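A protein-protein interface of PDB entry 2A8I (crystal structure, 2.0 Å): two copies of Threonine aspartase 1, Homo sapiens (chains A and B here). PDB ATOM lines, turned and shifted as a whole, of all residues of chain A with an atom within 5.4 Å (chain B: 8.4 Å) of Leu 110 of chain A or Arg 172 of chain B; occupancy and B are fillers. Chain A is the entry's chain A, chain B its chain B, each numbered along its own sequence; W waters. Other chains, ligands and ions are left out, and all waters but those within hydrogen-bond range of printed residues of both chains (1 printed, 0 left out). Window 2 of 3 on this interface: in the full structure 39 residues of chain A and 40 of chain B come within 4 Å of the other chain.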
ATOM      1  N   ASN A 108      22.178 -16.247  16.168  1.00  0.00           N
ATOM      2  CA  ASN A 108      23.279 -15.821  17.033  1.00  0.00           C
ATOM      3  C   ASN A 108      24.662 -16.221  16.495  1.00  0.00           C
ATOM      4  O   ASN A 108      24.792 -16.702  15.368  1.00  0.00           O
ATOM      5  CB  ASN A 108      23.098 -16.373  18.456  1.00  0.00           C
ATOM      6  CG  ASN A 108      23.314 -17.876  18.541  1.00  0.00           C
ATOM      7  OD1 ASN A 108      23.851 -18.497  17.626  1.00  0.00           O
ATOM      8  ND2 ASN A 108      22.913 -18.464  19.663  1.00  0.00           N
ATOM      9  N   LEU A 109      25.688 -16.020  17.315  1.00  0.00           N
ATOM     10  CA  LEU A 109      27.065 -16.325  16.943  1.00  0.00           C
ATOM     11  C   LEU A 109      27.252 -17.747  16.417  1.00  0.00           C
ATOM     12  O   LEU A 109      28.083 -17.989  15.542  1.00  0.00           O
ATOM     13  CB  LEU A 109      27.989 -16.117  18.149  1.00  0.00           C
ATOM     14  CG  LEU A 109      29.396 -15.554  17.916  1.00  0.00           C
ATOM     15  CD1 LEU A 109      30.286 -15.959  19.087  1.00  0.00           C
ATOM     16  CD2 LEU A 109      29.981 -16.068  16.612  1.00  0.00           C
ATOM     17  N   LEU A 110      26.490 -18.687  16.962  1.00  0.00           N
ATOM     18  CA  LEU A 110      26.581 -20.081  16.545  1.00  0.00           C
ATOM     19  C   LEU A 110      25.616 -20.427  15.420  1.00  0.00           C
ATOM     20  O   LEU A 110      25.561 -21.573  14.983  1.00  0.00           O
ATOM     21  CB  LEU A 110      26.310 -21.012  17.732  1.00  0.00           C
ATOM     22  CG  LEU A 110      27.471 -21.399  18.646  1.00  0.00           C
ATOM     23  CD1 LEU A 110      28.235 -20.166  19.090  1.00  0.00           C
ATOM     24  CD2 LEU A 110      26.924 -22.158  19.840  1.00  0.00           C
ATOM     25  N   GLY A 111      24.854 -19.443  14.954  1.00  0.00           N
ATOM     26  CA  GLY A 111      23.901 -19.703  13.888  1.00  0.00           C
ATOM     27  C   GLY A 111      22.638 -20.358  14.414  1.00  0.00           C
ATOM     28  O   GLY A 111      21.961 -21.097  13.695  1.00  0.00           O
ATOM     29  N   GLU A 112      22.326 -20.078  15.677  1.00  0.00           N
ATOM     30  CA  GLU A 112      21.146 -20.616  16.336  1.00  0.00           C
ATOM     31  C   GLU A 112      20.180 -19.511  16.761  1.00  0.00           C
ATOM     32  O   GLU A 112      20.570 -18.354  16.933  1.00  0.00           O
ATOM     33  CB  GLU A 112      21.562 -21.448  17.552  1.00  0.00           C
ATOM     34  CG  GLU A 112      21.962 -22.877  17.189  1.00  0.00           C
ATOM     35  CD  GLU A 112      22.742 -23.581  18.286  1.00  0.00           C
ATOM     36  OE1 GLU A 112      22.388 -23.431  19.479  1.00  0.00           O
ATOM     37  OE2 GLU A 112      23.709 -24.300  17.950  1.00  0.00           O
ATOM     38  N   PHE A 196      23.309 -14.372   8.276  1.00  0.00           N
ATOM     39  CA  PHE A 196      24.212 -14.982   9.243  1.00  0.00           C
ATOM     40  C   PHE A 196      25.592 -15.142   8.605  1.00  0.00           C
ATOM     41  O   PHE A 196      26.599 -14.652   9.131  1.00  0.00           O
ATOM     42  CB  PHE A 196      23.665 -16.347   9.676  1.00  0.00           C
ATOM     43  CG  PHE A 196      24.623 -17.151  10.515  1.00  0.00           C
ATOM     44  CD1 PHE A 196      25.051 -16.682  11.750  1.00  0.00           C
ATOM     45  CD2 PHE A 196      25.115 -18.371  10.052  1.00  0.00           C
ATOM     46  CE1 PHE A 196      25.961 -17.411  12.515  1.00  0.00           C
ATOM     47  CE2 PHE A 196      26.022 -19.108  10.803  1.00  0.00           C
ATOM     48  CZ  PHE A 196      26.450 -18.626  12.042  1.00  0.00           C
ATOM     49  N   LYS A 258      24.805 -12.309  18.499  1.00  0.00           N
ATOM     50  CA  LYS A 258      24.993 -12.378  19.936  1.00  0.00           C
ATOM     51  C   LYS A 258      25.546 -13.700  20.442  1.00  0.00           C
ATOM     52  O   LYS A 258      25.308 -14.779  19.882  1.00  0.00           O
ATOM     53  CB  LYS A 258      23.671 -12.089  20.645  1.00  0.00           C
ATOM     54  CG  LYS A 258      22.647 -13.190  20.482  1.00  0.00           C
ATOM     55  CD  LYS A 258      21.292 -12.796  21.040  1.00  0.00           C
ATOM     56  CE  LYS A 258      20.323 -13.951  20.901  1.00  0.00           C
ATOM     57  NZ  LYS A 258      18.973 -13.601  21.369  1.00  0.00           N
ATOM     58  N   HIS A 259      26.286 -13.597  21.533  1.00  0.00           N
ATOM     59  CA  HIS A 259      26.867 -14.762  22.159  1.00  0.00           C
ATOM     60  C   HIS A 259      25.722 -15.630  22.674  1.00  0.00           C
ATOM     61  O   HIS A 259      24.689 -15.117  23.094  1.00  0.00           O
ATOM     62  CB  HIS A 259      27.760 -14.327  23.323  1.00  0.00           C
ATOM     63  CG  HIS A 259      28.495 -15.457  23.964  1.00  0.00           C
ATOM     64  ND1 HIS A 259      27.865 -16.412  24.734  1.00  0.00           N
ATOM     65  CD2 HIS A 259      29.797 -15.825  23.896  1.00  0.00           C
ATOM     66  CE1 HIS A 259      28.746 -17.322  25.110  1.00  0.00           C
ATOM     67  NE2 HIS A 259      29.925 -16.989  24.616  1.00  0.00           N
ATOM     68  N   PRO A 260      25.870 -16.957  22.602  1.00  0.00           N
ATOM     69  CA  PRO A 260      24.803 -17.828  23.095  1.00  0.00           C
ATOM     70  C   PRO A 260      24.488 -17.447  24.551  1.00  0.00           C
ATOM     71  O   PRO A 260      25.380 -17.058  25.302  1.00  0.00           O
ATOM     72  CB  PRO A 260      25.428 -19.215  22.984  1.00  0.00           C
ATOM     73  CG  PRO A 260      26.267 -19.091  21.761  1.00  0.00           C
ATOM     74  CD  PRO A 260      26.920 -17.735  21.922  1.00  0.00           C
ATOM     75  N   LEU B 133      23.312 -20.428  35.937  1.00  0.00           N
ATOM     76  CA  LEU B 133      24.662 -20.874  35.622  1.00  0.00           C
ATOM     77  C   LEU B 133      25.062 -22.111  36.416  1.00  0.00           C
ATOM     78  O   LEU B 133      24.872 -22.162  37.632  1.00  0.00           O
ATOM     79  CB  LEU B 133      25.656 -19.755  35.921  1.00  0.00           C
ATOM     80  CG  LEU B 133      27.135 -20.087  35.719  1.00  0.00           C
ATOM     81  CD1 LEU B 133      27.376 -20.395  34.241  1.00  0.00           C
ATOM     82  CD2 LEU B 133      27.998 -18.913  36.183  1.00  0.00           C
ATOM     83  N   SER B 134      25.616 -23.097  35.717  1.00  0.00           N
ATOM     84  CA  SER B 134      26.084 -24.341  36.332  1.00  0.00           C
ATOM     85  C   SER B 134      27.545 -24.547  35.959  1.00  0.00           C
ATOM     86  O   SER B 134      28.050 -23.910  35.027  1.00  0.00           O
ATOM     87  CB  SER B 134      25.285 -25.534  35.812  1.00  0.00           C
ATOM     88  OG  SER B 134      23.901 -25.257  35.850  1.00  0.00           O
ATOM     89  N   ILE B 136      30.269 -23.655  37.454  1.00  0.00           N
ATOM     90  CA  ILE B 136      31.192 -22.592  37.829  1.00  0.00           C
ATOM     91  C   ILE B 136      31.122 -22.375  39.340  1.00  0.00           C
ATOM     92  O   ILE B 136      30.055 -22.097  39.889  1.00  0.00           O
ATOM     93  CB  ILE B 136      30.843 -21.275  37.098  1.00  0.00           C
ATOM     94  CG1 ILE B 136      30.971 -21.467  35.580  1.00  0.00           C
ATOM     95  CG2 ILE B 136      31.754 -20.154  37.574  1.00  0.00           C
ATOM     96  CD1 ILE B 136      32.380 -21.782  35.094  1.00  0.00           C
ATOM     97  N   VAL B 142      32.198 -14.443  37.396  1.00  0.00           N
ATOM     98  CA  VAL B 142      31.826 -14.410  35.992  1.00  0.00           C
ATOM     99  C   VAL B 142      31.101 -13.098  35.722  1.00  0.00           C
ATOM    100  O   VAL B 142      31.317 -12.463  34.691  1.00  0.00           O
ATOM    101  CB  VAL B 142      30.914 -15.595  35.624  1.00  0.00           C
ATOM    102  CG1 VAL B 142      30.563 -15.552  34.139  1.00  0.00           C
ATOM    103  CG2 VAL B 142      31.617 -16.900  35.952  1.00  0.00           C
ATOM    104  N   LEU B 165      24.280 -12.952  30.725  1.00  0.00           N
ATOM    105  CA  LEU B 165      24.319 -14.258  30.060  1.00  0.00           C
ATOM    106  C   LEU B 165      23.703 -15.326  30.950  1.00  0.00           C
ATOM    107  O   LEU B 165      23.867 -15.288  32.172  1.00  0.00           O
ATOM    108  CB  LEU B 165      25.764 -14.663  29.734  1.00  0.00           C
ATOM    109  CG  LEU B 165      26.563 -13.739  28.811  1.00  0.00           C
ATOM    110  CD1 LEU B 165      27.974 -14.291  28.644  1.00  0.00           C
ATOM    111  CD2 LEU B 165      25.858 -13.618  27.459  1.00  0.00           C
ATOM    112  N   VAL B 166      23.003 -16.281  30.345  1.00  0.00           N
ATOM    113  CA  VAL B 166      22.390 -17.364  31.112  1.00  0.00           C
ATOM    114  C   VAL B 166      22.720 -18.762  30.564  1.00  0.00           C
ATOM    115  O   VAL B 166      23.195 -18.910  29.436  1.00  0.00           O
ATOM    116  CB  VAL B 166      20.847 -17.223  31.157  1.00  0.00           C
ATOM    117  CG1 VAL B 166      20.461 -15.815  31.605  1.00  0.00           C
ATOM    118  CG2 VAL B 166      20.252 -17.557  29.802  1.00  0.00           C
ATOM    119  N   GLY B 167      22.465 -19.776  31.387  1.00  0.00           N
ATOM    120  CA  GLY B 167      22.678 -21.163  31.006  1.00  0.00           C
ATOM    121  C   GLY B 167      24.007 -21.587  30.407  1.00  0.00           C
ATOM    122  O   GLY B 167      25.071 -21.136  30.826  1.00  0.00           O
ATOM    123  N   GLU B 168      23.934 -22.481  29.424  1.00  0.00           N
ATOM    124  CA  GLU B 168      25.116 -23.000  28.743  1.00  0.00           C
ATOM    125  C   GLU B 168      26.004 -21.884  28.228  1.00  0.00           C
ATOM    126  O   GLU B 168      27.229 -21.977  28.281  1.00  0.00           O
ATOM    127  CB  GLU B 168      24.704 -23.870  27.559  1.00  0.00           C
ATOM    128  CG  GLU B 168      24.082 -25.209  27.922  1.00  0.00           C
ATOM    129  CD  GLU B 168      23.671 -25.999  26.685  1.00  0.00           C
ATOM    130  OE1 GLU B 168      24.544 -26.265  25.821  1.00  0.00           O
ATOM    131  OE2 GLU B 168      22.474 -26.346  26.573  1.00  0.00           O
ATOM    132  N   GLY B 169      25.369 -20.832  27.718  1.00  0.00           N
ATOM    133  CA  GLY B 169      26.098 -19.702  27.173  1.00  0.00           C
ATOM    134  C   GLY B 169      26.967 -18.993  28.189  1.00  0.00           C
ATOM    135  O   GLY B 169      28.100 -18.627  27.887  1.00  0.00           O
ATOM    136  N   ALA B 170      26.434 -18.785  29.388  1.00  0.00           N
ATOM    137  CA  ALA B 170      27.195 -18.125  30.437  1.00  0.00           C
ATOM    138  C   ALA B 170      28.358 -19.036  30.812  1.00  0.00           C
ATOM    139  O   ALA B 170      29.467 -18.570  31.056  1.00  0.00           O
ATOM    140  CB  ALA B 170      26.303 -17.867  31.654  1.00  0.00           C
ATOM    141  N   TYR B 171      28.092 -20.337  30.854  1.00  0.00           N
ATOM    142  CA  TYR B 171      29.114 -21.328  31.186  1.00  0.00           C
ATOM    143  C   TYR B 171      30.241 -21.308  30.148  1.00  0.00           C
ATOM    144  O   TYR B 171      31.423 -21.265  30.495  1.00  0.00           O
ATOM    145  CB  TYR B 171      28.489 -22.724  31.226  1.00  0.00           C
ATOM    146  CG  TYR B 171      29.497 -23.843  31.339  1.00  0.00           C
ATOM    147  CD1 TYR B 171      30.111 -24.133  32.554  1.00  0.00           C
ATOM    148  CD2 TYR B 171      29.845 -24.608  30.224  1.00  0.00           C
ATOM    149  CE1 TYR B 171      31.047 -25.156  32.660  1.00  0.00           C
ATOM    150  CE2 TYR B 171      30.783 -25.638  30.316  1.00  0.00           C
ATOM    151  CZ  TYR B 171      31.377 -25.905  31.538  1.00  0.00           C
ATOM    152  OH  TYR B 171      32.298 -26.920  31.650  1.00  0.00           O
ATOM    153  N   ARG B 172      29.866 -21.344  28.872  1.00  0.00           N
ATOM    154  CA  ARG B 172      30.850 -21.331  27.791  1.00  0.00           C
ATOM    155  C   ARG B 172      31.709 -20.074  27.872  1.00  0.00           C
ATOM    156  O   ARG B 172      32.934 -20.123  27.745  1.00  0.00           O
ATOM    157  CB  ARG B 172      30.155 -21.357  26.423  1.00  0.00           C
ATOM    158  CG  ARG B 172      31.151 -21.306  25.263  1.00  0.00           C
ATOM    159  CD  ARG B 172      30.606 -20.578  24.032  1.00  0.00           C
ATOM    160  NE  ARG B 172      31.604 -20.528  22.959  1.00  0.00           N
ATOM    161  CZ  ARG B 172      31.471 -19.826  21.836  1.00  0.00           C
ATOM    162  NH1 ARG B 172      30.379 -19.098  21.623  1.00  0.00           N
ATOM    163  NH2 ARG B 172      32.433 -19.847  20.920  1.00  0.00           N
ATOM    164  N   TRP B 173      31.045 -18.945  28.078  1.00  0.00           N
ATOM    165  CA  TRP B 173      31.713 -17.656  28.164  1.00  0.00           C
ATOM    166  C   TRP B 173      32.748 -17.649  29.293  1.00  0.00           C
ATOM    167  O   TRP B 173      33.864 -17.165  29.111  1.00  0.00           O
ATOM    168  CB  TRP B 173      30.671 -16.556  28.387  1.00  0.00           C
ATOM    169  CG  TRP B 173      31.181 -15.188  28.114  1.00  0.00           C
ATOM    170  CD1 TRP B 173      31.121 -14.512  26.927  1.00  0.00           C
ATOM    171  CD2 TRP B 173      31.866 -14.331  29.031  1.00  0.00           C
ATOM    172  NE1 TRP B 173      31.728 -13.288  27.052  1.00  0.00           N
ATOM    173  CE2 TRP B 173      32.196 -13.150  28.332  1.00  0.00           C
ATOM    174  CE3 TRP B 173      32.237 -14.447  30.378  1.00  0.00           C
ATOM    175  CZ2 TRP B 173      32.882 -12.086  28.936  1.00  0.00           C
ATOM    176  CZ3 TRP B 173      32.921 -13.389  30.980  1.00  0.00           C
ATOM    177  CH2 TRP B 173      33.235 -12.227  30.258  1.00  0.00           C
ATOM    178  N   ALA B 174      32.375 -18.189  30.452  1.00  0.00           N
ATOM    179  CA  ALA B 174      33.273 -18.247  31.606  1.00  0.00           C
ATOM    180  C   ALA B 174      34.522 -19.071  31.285  1.00  0.00           C
ATOM    181  O   ALA B 174      35.650 -18.643  31.544  1.00  0.00           O
ATOM    182  CB  ALA B 174      32.546 -18.849  32.805  1.00  0.00           C
ATOM    183  N   VAL B 175      34.311 -20.254  30.722  1.00  0.00           N
ATOM    184  CA  VAL B 175      35.416 -21.133  30.360  1.00  0.00           C
ATOM    185  C   VAL B 175      36.330 -20.491  29.312  1.00  0.00           C
ATOM    186  O   VAL B 175      37.554 -20.566  29.419  1.00  0.00           O
ATOM    187  CB  VAL B 175      34.885 -22.482  29.827  1.00  0.00           C
ATOM    188  CG1 VAL B 175      36.036 -23.330  29.276  1.00  0.00           C
ATOM    189  CG2 VAL B 175      34.166 -23.219  30.950  1.00  0.00           C
ATOM    190  N   ASP B 176      35.730 -19.847  28.318  1.00  0.00           N
ATOM    191  CA  ASP B 176      36.488 -19.196  27.251  1.00  0.00           C
ATOM    192  C   ASP B 176      37.364 -18.047  27.734  1.00  0.00           C
ATOM    193  O   ASP B 176      38.358 -17.710  27.085  1.00  0.00           O
ATOM    194  CB  ASP B 176      35.552 -18.680  26.156  1.00  0.00           C
ATOM    195  CG  ASP B 176      34.963 -19.798  25.314  1.00  0.00           C
ATOM    196  OD1 ASP B 176      35.469 -20.940  25.380  1.00  0.00           O
ATOM    197  OD2 ASP B 176      33.997 -19.531  24.571  1.00  0.00           O
ATOM    198  N   HIS B 177      37.002 -17.438  28.861  1.00  0.00           N
ATOM    199  CA  HIS B 177      37.799 -16.341  29.397  1.00  0.00           C
ATOM    200  C   HIS B 177      38.738 -16.757  30.521  1.00  0.00           C
ATOM    201  O   HIS B 177      39.163 -15.927  31.314  1.00  0.00           O
ATOM    202  CB  HIS B 177      36.902 -15.183  29.854  1.00  0.00           C
ATOM    203  CG  HIS B 177      36.218 -14.482  28.722  1.00  0.00           C
ATOM    204  ND1 HIS B 177      35.281 -15.103  27.922  1.00  0.00           N
ATOM    205  CD2 HIS B 177      36.384 -13.238  28.212  1.00  0.00           C
ATOM    206  CE1 HIS B 177      34.904 -14.274  26.965  1.00  0.00           C
ATOM    207  NE2 HIS B 177      35.557 -13.136  27.118  1.00  0.00           N
ATOM    208  N   GLY B 178      39.054 -18.048  30.588  1.00  0.00           N
ATOM    209  CA  GLY B 178      39.995 -18.526  31.586  1.00  0.00           C
ATOM    210  C   GLY B 178      39.508 -18.957  32.959  1.00  0.00           C
ATOM    211  O   GLY B 178      40.323 -19.196  33.846  1.00  0.00           O
ATOM    212  N   ILE B 179      38.200 -19.040  33.151  1.00  0.00           N
ATOM    213  CA  ILE B 179      37.652 -19.472  34.430  1.00  0.00           C
ATOM    214  C   ILE B 179      37.363 -20.965  34.277  1.00  0.00           C
ATOM    215  O   ILE B 179      36.461 -21.360  33.541  1.00  0.00           O
ATOM    216  CB  ILE B 179      36.351 -18.708  34.759  1.00  0.00           C
ATOM    217  CG1 ILE B 179      36.630 -17.201  34.764  1.00  0.00           C
ATOM    218  CG2 ILE B 179      35.799 -19.160  36.103  1.00  0.00           C
ATOM    219  CD1 ILE B 179      35.392 -16.337  34.992  1.00  0.00           C
HETATM  220  O   HOH W   1      32.785 -17.212  24.328  1.00  0.00           O
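Among the printed residues, pairs that only touch across the chains: Leu 110 of chain A with Arg 172 of chain B (3.5 Å), His 259 of chain A with Gly 169 of chain B (3.1 Å), His 259 of chain A with Arg 172 of chain B (3.7 Å), His 259 of chain A with Trp 173 of chain B (3.6 Å), Pro 260 of chain A with Gly 169 of chain B (3.3 Å) and Pro 260 of chain A with Arg 172 of chain B (3.7 Å).
Of chain B, only Arg 172 comes within 4 Å of Leu 110 of chain A. Of chain A, only Leu 110 (3.5 Å), His 259 (3.7 Å) and Pro 260 (3.7 Å) come within 4 Å of Arg 172 of chain B. No residue of chain B comes within 4 Å of Gly 111 of chain A. Of the printed residues of chain B, His 259 of chain A touches Gly 169 (3.1 Å), Arg 172 (3.7 Å) and Trp 173 (3.6 Å). Of the printed residues of chain A, Gly 169 of chain B touches His 259 (3.1 Å) and Pro 260 (3.3 Å). The nearest residue of chain A that does not touch Arg 172 of chain B is Leu 109 of chain A (4.04 Å). The nearest printed residue of chain B that does not touch His 259 of chain A is Leu 165 of chain B (4.4 Å).
Of the 19 printed residues of chain B, 3 touch a printed residue of chain A. Among the printed residues, 6 pairs touch across the chains. Among the printed residues, no Asp or Glu carboxylate lies within 4 Å of a Lys or Arg side-chain nitrogen of the other chain.
No position is printed for both chains. Of the 6 pairs that touch across the chains among the printed residues, none has its exchanged pair printed and touching as well.
OD2 of Asp 176 of chain B lies within salt-bridge range of NE of Arg 172 of chain B. O of Trp 173 of chain B sits at hydrogen-bond distance from ND1 of His 177 of chain B (2.8 Å). The backbone NH of Leu 110 of chain A lies within hydrogen-bond range of the side-chain amide oxygen of Asn 108 of chain A.
Water W1 lies within hydrogen-bond range of OD2 of Asp 176 of chain B (2.6 Å) and NE2 of His 259 of chain A (2.9 Å).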
